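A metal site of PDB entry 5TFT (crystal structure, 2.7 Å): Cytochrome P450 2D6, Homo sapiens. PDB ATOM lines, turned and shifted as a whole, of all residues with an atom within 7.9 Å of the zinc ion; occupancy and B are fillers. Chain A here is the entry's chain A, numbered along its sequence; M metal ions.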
ATOM      1  N   TRP A 130       2.945 -38.933   4.405  1.00  0.00           N
ATOM      2  CA  TRP A 130       4.089 -39.216   5.275  1.00  0.00           C
ATOM      3  C   TRP A 130       4.076 -40.659   5.775  1.00  0.00           C
ATOM      4  O   TRP A 130       5.134 -41.254   5.967  1.00  0.00           O
ATOM      5  CB  TRP A 130       4.117 -38.258   6.470  1.00  0.00           C
ATOM      6  CG  TRP A 130       4.737 -36.923   6.171  1.00  0.00           C
ATOM      7  CD1 TRP A 130       5.929 -36.699   5.556  1.00  0.00           C
ATOM      8  CD2 TRP A 130       4.201 -35.638   6.504  1.00  0.00           C
ATOM      9  NE1 TRP A 130       6.161 -35.339   5.471  1.00  0.00           N
ATOM     10  CE2 TRP A 130       5.112 -34.669   6.039  1.00  0.00           C
ATOM     11  CE3 TRP A 130       3.030 -35.204   7.136  1.00  0.00           C
ATOM     12  CZ2 TRP A 130       4.904 -33.299   6.194  1.00  0.00           C
ATOM     13  CZ3 TRP A 130       2.815 -33.846   7.286  1.00  0.00           C
ATOM     14  CH2 TRP A 130       3.751 -32.912   6.825  1.00  0.00           C
ATOM     15  N   ALA A 165       6.984 -37.326  14.096  1.00  0.00           N
ATOM     16  CA  ALA A 165       7.904 -36.238  13.789  1.00  0.00           C
ATOM     17  C   ALA A 165       7.465 -35.503  12.530  1.00  0.00           C
ATOM     18  O   ALA A 165       7.715 -34.306  12.390  1.00  0.00           O
ATOM     19  CB  ALA A 165       9.320 -36.771  13.631  1.00  0.00           C
ATOM     20  N   SER A 166       6.815 -36.217  11.631  1.00  0.00           N
ATOM     21  CA  SER A 166       6.291 -35.629  10.403  1.00  0.00           C
ATOM     22  C   SER A 166       5.114 -34.711  10.701  1.00  0.00           C
ATOM     23  O   SER A 166       4.850 -33.770   9.957  1.00  0.00           O
ATOM     24  CB  SER A 166       5.875 -36.716   9.413  1.00  0.00           C
ATOM     25  OG  SER A 166       6.981 -37.540   9.076  1.00  0.00           O
ATOM     26  N   LEU A 167       4.407 -34.990  11.785  1.00  0.00           N
ATOM     27  CA  LEU A 167       3.259 -34.177  12.162  1.00  0.00           C
ATOM     28  C   LEU A 167       3.652 -33.058  13.111  1.00  0.00           C
ATOM     29  O   LEU A 167       3.111 -31.948  13.044  1.00  0.00           O
ATOM     30  CB  LEU A 167       2.159 -35.039  12.780  1.00  0.00           C
ATOM     31  CG  LEU A 167       1.497 -36.001  11.782  1.00  0.00           C
ATOM     32  CD1 LEU A 167       0.271 -36.655  12.380  1.00  0.00           C
ATOM     33  CD2 LEU A 167       1.133 -35.270  10.489  1.00  0.00           C
ATOM     34  N   THR A 168       4.599 -33.331  14.006  1.00  0.00           N
ATOM     35  CA  THR A 168       5.092 -32.307  14.915  1.00  0.00           C
ATOM     36  C   THR A 168       6.053 -31.344  14.215  1.00  0.00           C
ATOM     37  O   THR A 168       5.763 -30.148  14.114  1.00  0.00           O
ATOM     38  CB  THR A 168       5.802 -32.921  16.130  1.00  0.00           C
ATOM     39  OG1 THR A 168       6.940 -33.677  15.695  1.00  0.00           O
ATOM     40  CG2 THR A 168       4.856 -33.819  16.901  1.00  0.00           C
ATOM     41  N   CYS A 169       7.170 -31.853  13.709  1.00  0.00           N
ATOM     42  CA  CYS A 169       8.224 -30.985  13.178  1.00  0.00           C
ATOM     43  C   CYS A 169       8.376 -31.039  11.646  1.00  0.00           C
ATOM     44  O   CYS A 169       9.305 -30.457  11.096  1.00  0.00           O
ATOM     45  CB  CYS A 169       9.572 -31.327  13.826  1.00  0.00           C
ATOM     46  SG  CYS A 169       9.655 -31.054  15.603  1.00  0.00           S
ATOM     47  N   GLY A 170       7.466 -31.734  10.979  1.00  0.00           N
ATOM     48  CA  GLY A 170       7.468 -31.781   9.515  1.00  0.00           C
ATOM     49  C   GLY A 170       8.703 -32.416   8.893  1.00  0.00           C
ATOM     50  O   GLY A 170       9.150 -31.999   7.831  1.00  0.00           O
ATOM     51  N   ARG A 171       9.241 -33.434   9.555  1.00  0.00           N
ATOM     52  CA  ARG A 171      10.427 -34.116   9.048  1.00  0.00           C
ATOM     53  C   ARG A 171      10.466 -35.580   9.483  1.00  0.00           C
ATOM     54  O   ARG A 171       9.728 -35.987  10.376  1.00  0.00           O
ATOM     55  CB  ARG A 171      11.707 -33.425   9.518  1.00  0.00           C
ATOM     56  CG  ARG A 171      12.043 -33.741  10.968  1.00  0.00           C
ATOM     57  CD  ARG A 171      13.468 -33.355  11.313  1.00  0.00           C
ATOM     58  NE  ARG A 171      14.452 -34.150  10.576  1.00  0.00           N
ATOM     59  CZ  ARG A 171      15.764 -34.041  10.723  1.00  0.00           C
ATOM     60  NH1 ARG A 171      16.262 -33.155  11.578  1.00  0.00           N
ATOM     61  NH2 ARG A 171      16.582 -34.800  10.008  1.00  0.00           N
ATOM     62  N   HIS A 236      14.077 -26.374  14.466  1.00  0.00           N
ATOM     63  CA  HIS A 236      12.852 -26.225  13.692  1.00  0.00           C
ATOM     64  C   HIS A 236      12.341 -24.788  13.683  1.00  0.00           C
ATOM     65  O   HIS A 236      11.736 -24.343  12.709  1.00  0.00           O
ATOM     66  CB  HIS A 236      11.768 -27.160  14.234  1.00  0.00           C
ATOM     67  CG  HIS A 236      10.506 -27.135  13.429  1.00  0.00           C
ATOM     68  ND1 HIS A 236       9.255 -27.201  14.006  1.00  0.00           N
ATOM     69  CD2 HIS A 236      10.297 -27.068  12.095  1.00  0.00           C
ATOM     70  CE1 HIS A 236       8.340 -27.165  13.064  1.00  0.00           C
ATOM     71  NE2 HIS A 236       8.939 -27.091  11.894  1.00  0.00           N
ATOM     72  N   ARG A 237      12.594 -24.068  14.770  1.00  0.00           N
ATOM     73  CA  ARG A 237      12.165 -22.678  14.878  1.00  0.00           C
ATOM     74  C   ARG A 237      12.929 -21.809  13.878  1.00  0.00           C
ATOM     75  O   ARG A 237      12.413 -20.806  13.399  1.00  0.00           O
ATOM     76  CB  ARG A 237      12.370 -22.165  16.301  1.00  0.00           C
ATOM     77  CG  ARG A 237      11.682 -20.829  16.584  1.00  0.00           C
ATOM     78  CD  ARG A 237      12.037 -20.310  17.972  1.00  0.00           C
ATOM     79  NE  ARG A 237      11.619 -21.214  19.040  1.00  0.00           N
ATOM     80  CZ  ARG A 237      10.501 -21.074  19.747  1.00  0.00           C
ATOM     81  NH1 ARG A 237       9.692 -20.054  19.509  1.00  0.00           N
ATOM     82  NH2 ARG A 237      10.213 -21.944  20.700  1.00  0.00           N
ATOM     83  N   THR A 239      14.036 -22.780  10.797  1.00  0.00           N
ATOM     84  CA  THR A 239      13.640 -23.031   9.418  1.00  0.00           C
ATOM     85  C   THR A 239      12.179 -22.681   9.130  1.00  0.00           C
ATOM     86  O   THR A 239      11.732 -22.732   7.986  1.00  0.00           O
ATOM     87  CB  THR A 239      13.866 -24.505   9.037  1.00  0.00           C
ATOM     88  OG1 THR A 239      13.107 -25.352   9.920  1.00  0.00           O
ATOM     89  CG2 THR A 239      15.336 -24.872   9.130  1.00  0.00           C
ATOM     90  N   TRP A 240      11.439 -22.310  10.182  1.00  0.00           N
ATOM     91  CA  TRP A 240      10.016 -21.978  10.043  1.00  0.00           C
ATOM     92  C   TRP A 240       9.799 -20.710   9.213  1.00  0.00           C
ATOM     93  O   TRP A 240      10.408 -19.672   9.490  1.00  0.00           O
ATOM     94  CB  TRP A 240       9.383 -21.808  11.428  1.00  0.00           C
ATOM     95  CG  TRP A 240       8.000 -21.254  11.390  1.00  0.00           C
ATOM     96  CD1 TRP A 240       6.983 -21.625  10.553  1.00  0.00           C
ATOM     97  CD2 TRP A 240       7.465 -20.213  12.219  1.00  0.00           C
ATOM     98  NE1 TRP A 240       5.853 -20.888  10.818  1.00  0.00           N
ATOM     99  CE2 TRP A 240       6.123 -20.014  11.833  1.00  0.00           C
ATOM    100  CE3 TRP A 240       7.986 -19.438  13.257  1.00  0.00           C
ATOM    101  CZ2 TRP A 240       5.303 -19.068  12.441  1.00  0.00           C
ATOM    102  CZ3 TRP A 240       7.175 -18.494  13.861  1.00  0.00           C
ATOM    103  CH2 TRP A 240       5.851 -18.316  13.456  1.00  0.00           C
ATOM    104  N   ASP A 241       8.926 -20.808   8.217  1.00  0.00           N
ATOM    105  CA  ASP A 241       8.578 -19.660   7.379  1.00  0.00           C
ATOM    106  C   ASP A 241       7.147 -19.202   7.649  1.00  0.00           C
ATOM    107  O   ASP A 241       6.196 -19.807   7.156  1.00  0.00           O
ATOM    108  CB  ASP A 241       8.755 -20.014   5.893  1.00  0.00           C
ATOM    109  CG  ASP A 241       8.564 -18.812   4.979  1.00  0.00           C
ATOM    110  OD1 ASP A 241       8.348 -19.004   3.761  1.00  0.00           O
ATOM    111  OD2 ASP A 241       8.637 -17.662   5.469  1.00  0.00           O
ATOM    112  N   PRO A 246       1.210 -23.242   7.808  1.00  0.00           N
ATOM    113  CA  PRO A 246       1.970 -24.202   8.617  1.00  0.00           C
ATOM    114  C   PRO A 246       2.107 -25.584   7.967  1.00  0.00           C
ATOM    115  O   PRO A 246       1.116 -26.169   7.542  1.00  0.00           O
ATOM    116  CB  PRO A 246       1.153 -24.293   9.905  1.00  0.00           C
ATOM    117  CG  PRO A 246       0.467 -22.962   9.995  1.00  0.00           C
ATOM    118  CD  PRO A 246       0.132 -22.601   8.583  1.00  0.00           C
ATOM    119  N   ARG A 247       3.327 -26.088   7.890  1.00  0.00           N
ATOM    120  CA  ARG A 247       3.592 -27.420   7.352  1.00  0.00           C
ATOM    121  C   ARG A 247       3.306 -28.514   8.372  1.00  0.00           C
ATOM    122  O   ARG A 247       3.064 -29.665   8.012  1.00  0.00           O
ATOM    123  CB  ARG A 247       5.041 -27.540   6.890  1.00  0.00           C
ATOM    124  CG  ARG A 247       5.413 -26.727   5.668  1.00  0.00           C
ATOM    125  CD  ARG A 247       6.759 -27.171   5.122  1.00  0.00           C
ATOM    126  NE  ARG A 247       6.726 -28.551   4.639  1.00  0.00           N
ATOM    127  CZ  ARG A 247       7.162 -29.610   5.316  1.00  0.00           C
ATOM    128  NH1 ARG A 247       7.668 -29.468   6.531  1.00  0.00           N
ATOM    129  NH2 ARG A 247       7.084 -30.822   4.771  1.00  0.00           N
ATOM    130  N   ASP A 248       3.356 -28.144   9.650  1.00  0.00           N
ATOM    131  CA  ASP A 248       3.240 -29.117  10.726  1.00  0.00           C
ATOM    132  C   ASP A 248       2.604 -28.490  11.975  1.00  0.00           C
ATOM    133  O   ASP A 248       2.318 -27.296  11.992  1.00  0.00           O
ATOM    134  CB  ASP A 248       4.609 -29.708  11.048  1.00  0.00           C
ATOM    135  CG  ASP A 248       5.682 -28.646  11.195  1.00  0.00           C
ATOM    136  OD1 ASP A 248       5.537 -27.766  12.058  1.00  0.00           O
ATOM    137  OD2 ASP A 248       6.674 -28.687  10.433  1.00  0.00           O
ATOM    138  N   LEU A 249       2.403 -29.295  13.002  1.00  0.00           N
ATOM    139  CA  LEU A 249       1.699 -28.855  14.207  1.00  0.00           C
ATOM    140  C   LEU A 249       2.494 -27.796  14.966  1.00  0.00           C
ATOM    141  O   LEU A 249       1.917 -26.856  15.520  1.00  0.00           O
ATOM    142  CB  LEU A 249       1.402 -30.041  15.112  1.00  0.00           C
ATOM    143  CG  LEU A 249       0.665 -29.751  16.424  1.00  0.00           C
ATOM    144  CD1 LEU A 249      -0.433 -30.775  16.646  1.00  0.00           C
ATOM    145  CD2 LEU A 249       1.620 -29.740  17.607  1.00  0.00           C
ATOM    146  N   THR A 250       3.812 -27.956  14.995  1.00  0.00           N
ATOM    147  CA  THR A 250       4.678 -27.014  15.701  1.00  0.00           C
ATOM    148  C   THR A 250       4.582 -25.628  15.079  1.00  0.00           C
ATOM    149  O   THR A 250       4.501 -24.617  15.798  1.00  0.00           O
ATOM    150  CB  THR A 250       6.143 -27.488  15.703  1.00  0.00           C
ATOM    151  OG1 THR A 250       6.232 -28.789  16.320  1.00  0.00           O
ATOM    152  CG2 THR A 250       7.024 -26.528  16.467  1.00  0.00           C
ATOM    153  N   GLU A 251       4.591 -25.563  13.753  1.00  0.00           N
ATOM    154  CA  GLU A 251       4.466 -24.289  13.044  1.00  0.00           C
ATOM    155  C   GLU A 251       3.109 -23.653  13.308  1.00  0.00           C
ATOM    156  O   GLU A 251       3.005 -22.440  13.496  1.00  0.00           O
ATOM    157  CB  GLU A 251       4.681 -24.483  11.543  1.00  0.00           C
ATOM    158  CG  GLU A 251       6.109 -24.858  11.169  1.00  0.00           C
ATOM    159  CD  GLU A 251       6.311 -25.004   9.677  1.00  0.00           C
ATOM    160  OE1 GLU A 251       5.528 -24.402   8.910  1.00  0.00           O
ATOM    161  OE2 GLU A 251       7.253 -25.716   9.271  1.00  0.00           O
ATOM    162  N   ALA A 252       2.075 -24.483  13.321  1.00  0.00           N
ATOM    163  CA  ALA A 252       0.728 -24.024  13.635  1.00  0.00           C
ATOM    164  C   ALA A 252       0.668 -23.521  15.082  1.00  0.00           C
ATOM    165  O   ALA A 252      -0.046 -22.560  15.391  1.00  0.00           O
ATOM    166  CB  ALA A 252      -0.280 -25.142  13.424  1.00  0.00           C
ATOM    167  N   LEU A 254       3.350 -22.312  16.714  1.00  0.00           N
ATOM    168  CA  LEU A 254       4.147 -21.086  16.705  1.00  0.00           C
ATOM    169  C   LEU A 254       3.335 -19.902  16.199  1.00  0.00           C
ATOM    170  O   LEU A 254       3.429 -18.803  16.737  1.00  0.00           O
ATOM    171  CB  LEU A 254       5.408 -21.262  15.844  1.00  0.00           C
ATOM    172  CG  LEU A 254       6.493 -22.201  16.382  1.00  0.00           C
ATOM    173  CD1 LEU A 254       7.556 -22.451  15.339  1.00  0.00           C
ATOM    174  CD2 LEU A 254       7.114 -21.646  17.665  1.00  0.00           C
HETATM  175 ZN    ZN M   1       8.067 -27.284  10.148  1.00  0.00          ZN
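A ring nitrogen (NE2) of His 236 sits close to the backbone carbonyl oxygen (O) of Cys 169, 3.5 Å away. The side-chain hydroxyl (OG1) of Thr 239 is in hydrogen-bond range of the backbone carbonyl oxygen (O) of His 236. The side-chain carboxylate (OE1) of Glu 251 lies within hydrogen-bond range of the backbone NH (N) of Arg 247, at 3.0 Å. N of Gly 170 lies close to OD2 of Asp 248 (3.2 Å). The side-chain carboxylate (OD1) of Asp 248 sits close to the backbone NH (N) of Thr 250 (3.4 Å). SG of Cys 169 lies within hydrogen-bond range of OG1 of Thr 168 (3.8 Å).
Cys 169 touches the zinc ion. Within 4 Å of the zinc ion: Cys 169, His 236, Asp 248 and Glu 251. Along chain A the residues within 4 Å of the zinc ion span positions 169 to 251. The nearest printed residue that does not touch the zinc ion is Arg 247 (4.2 Å).
The zinc ion is bound by NE2 of His 236 (2.0 Å). The zinc ion is bound by OE2 of Glu 251 (2.0 Å). The zinc ion is bound by OD2 of Asp 248 (2.0 Å).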
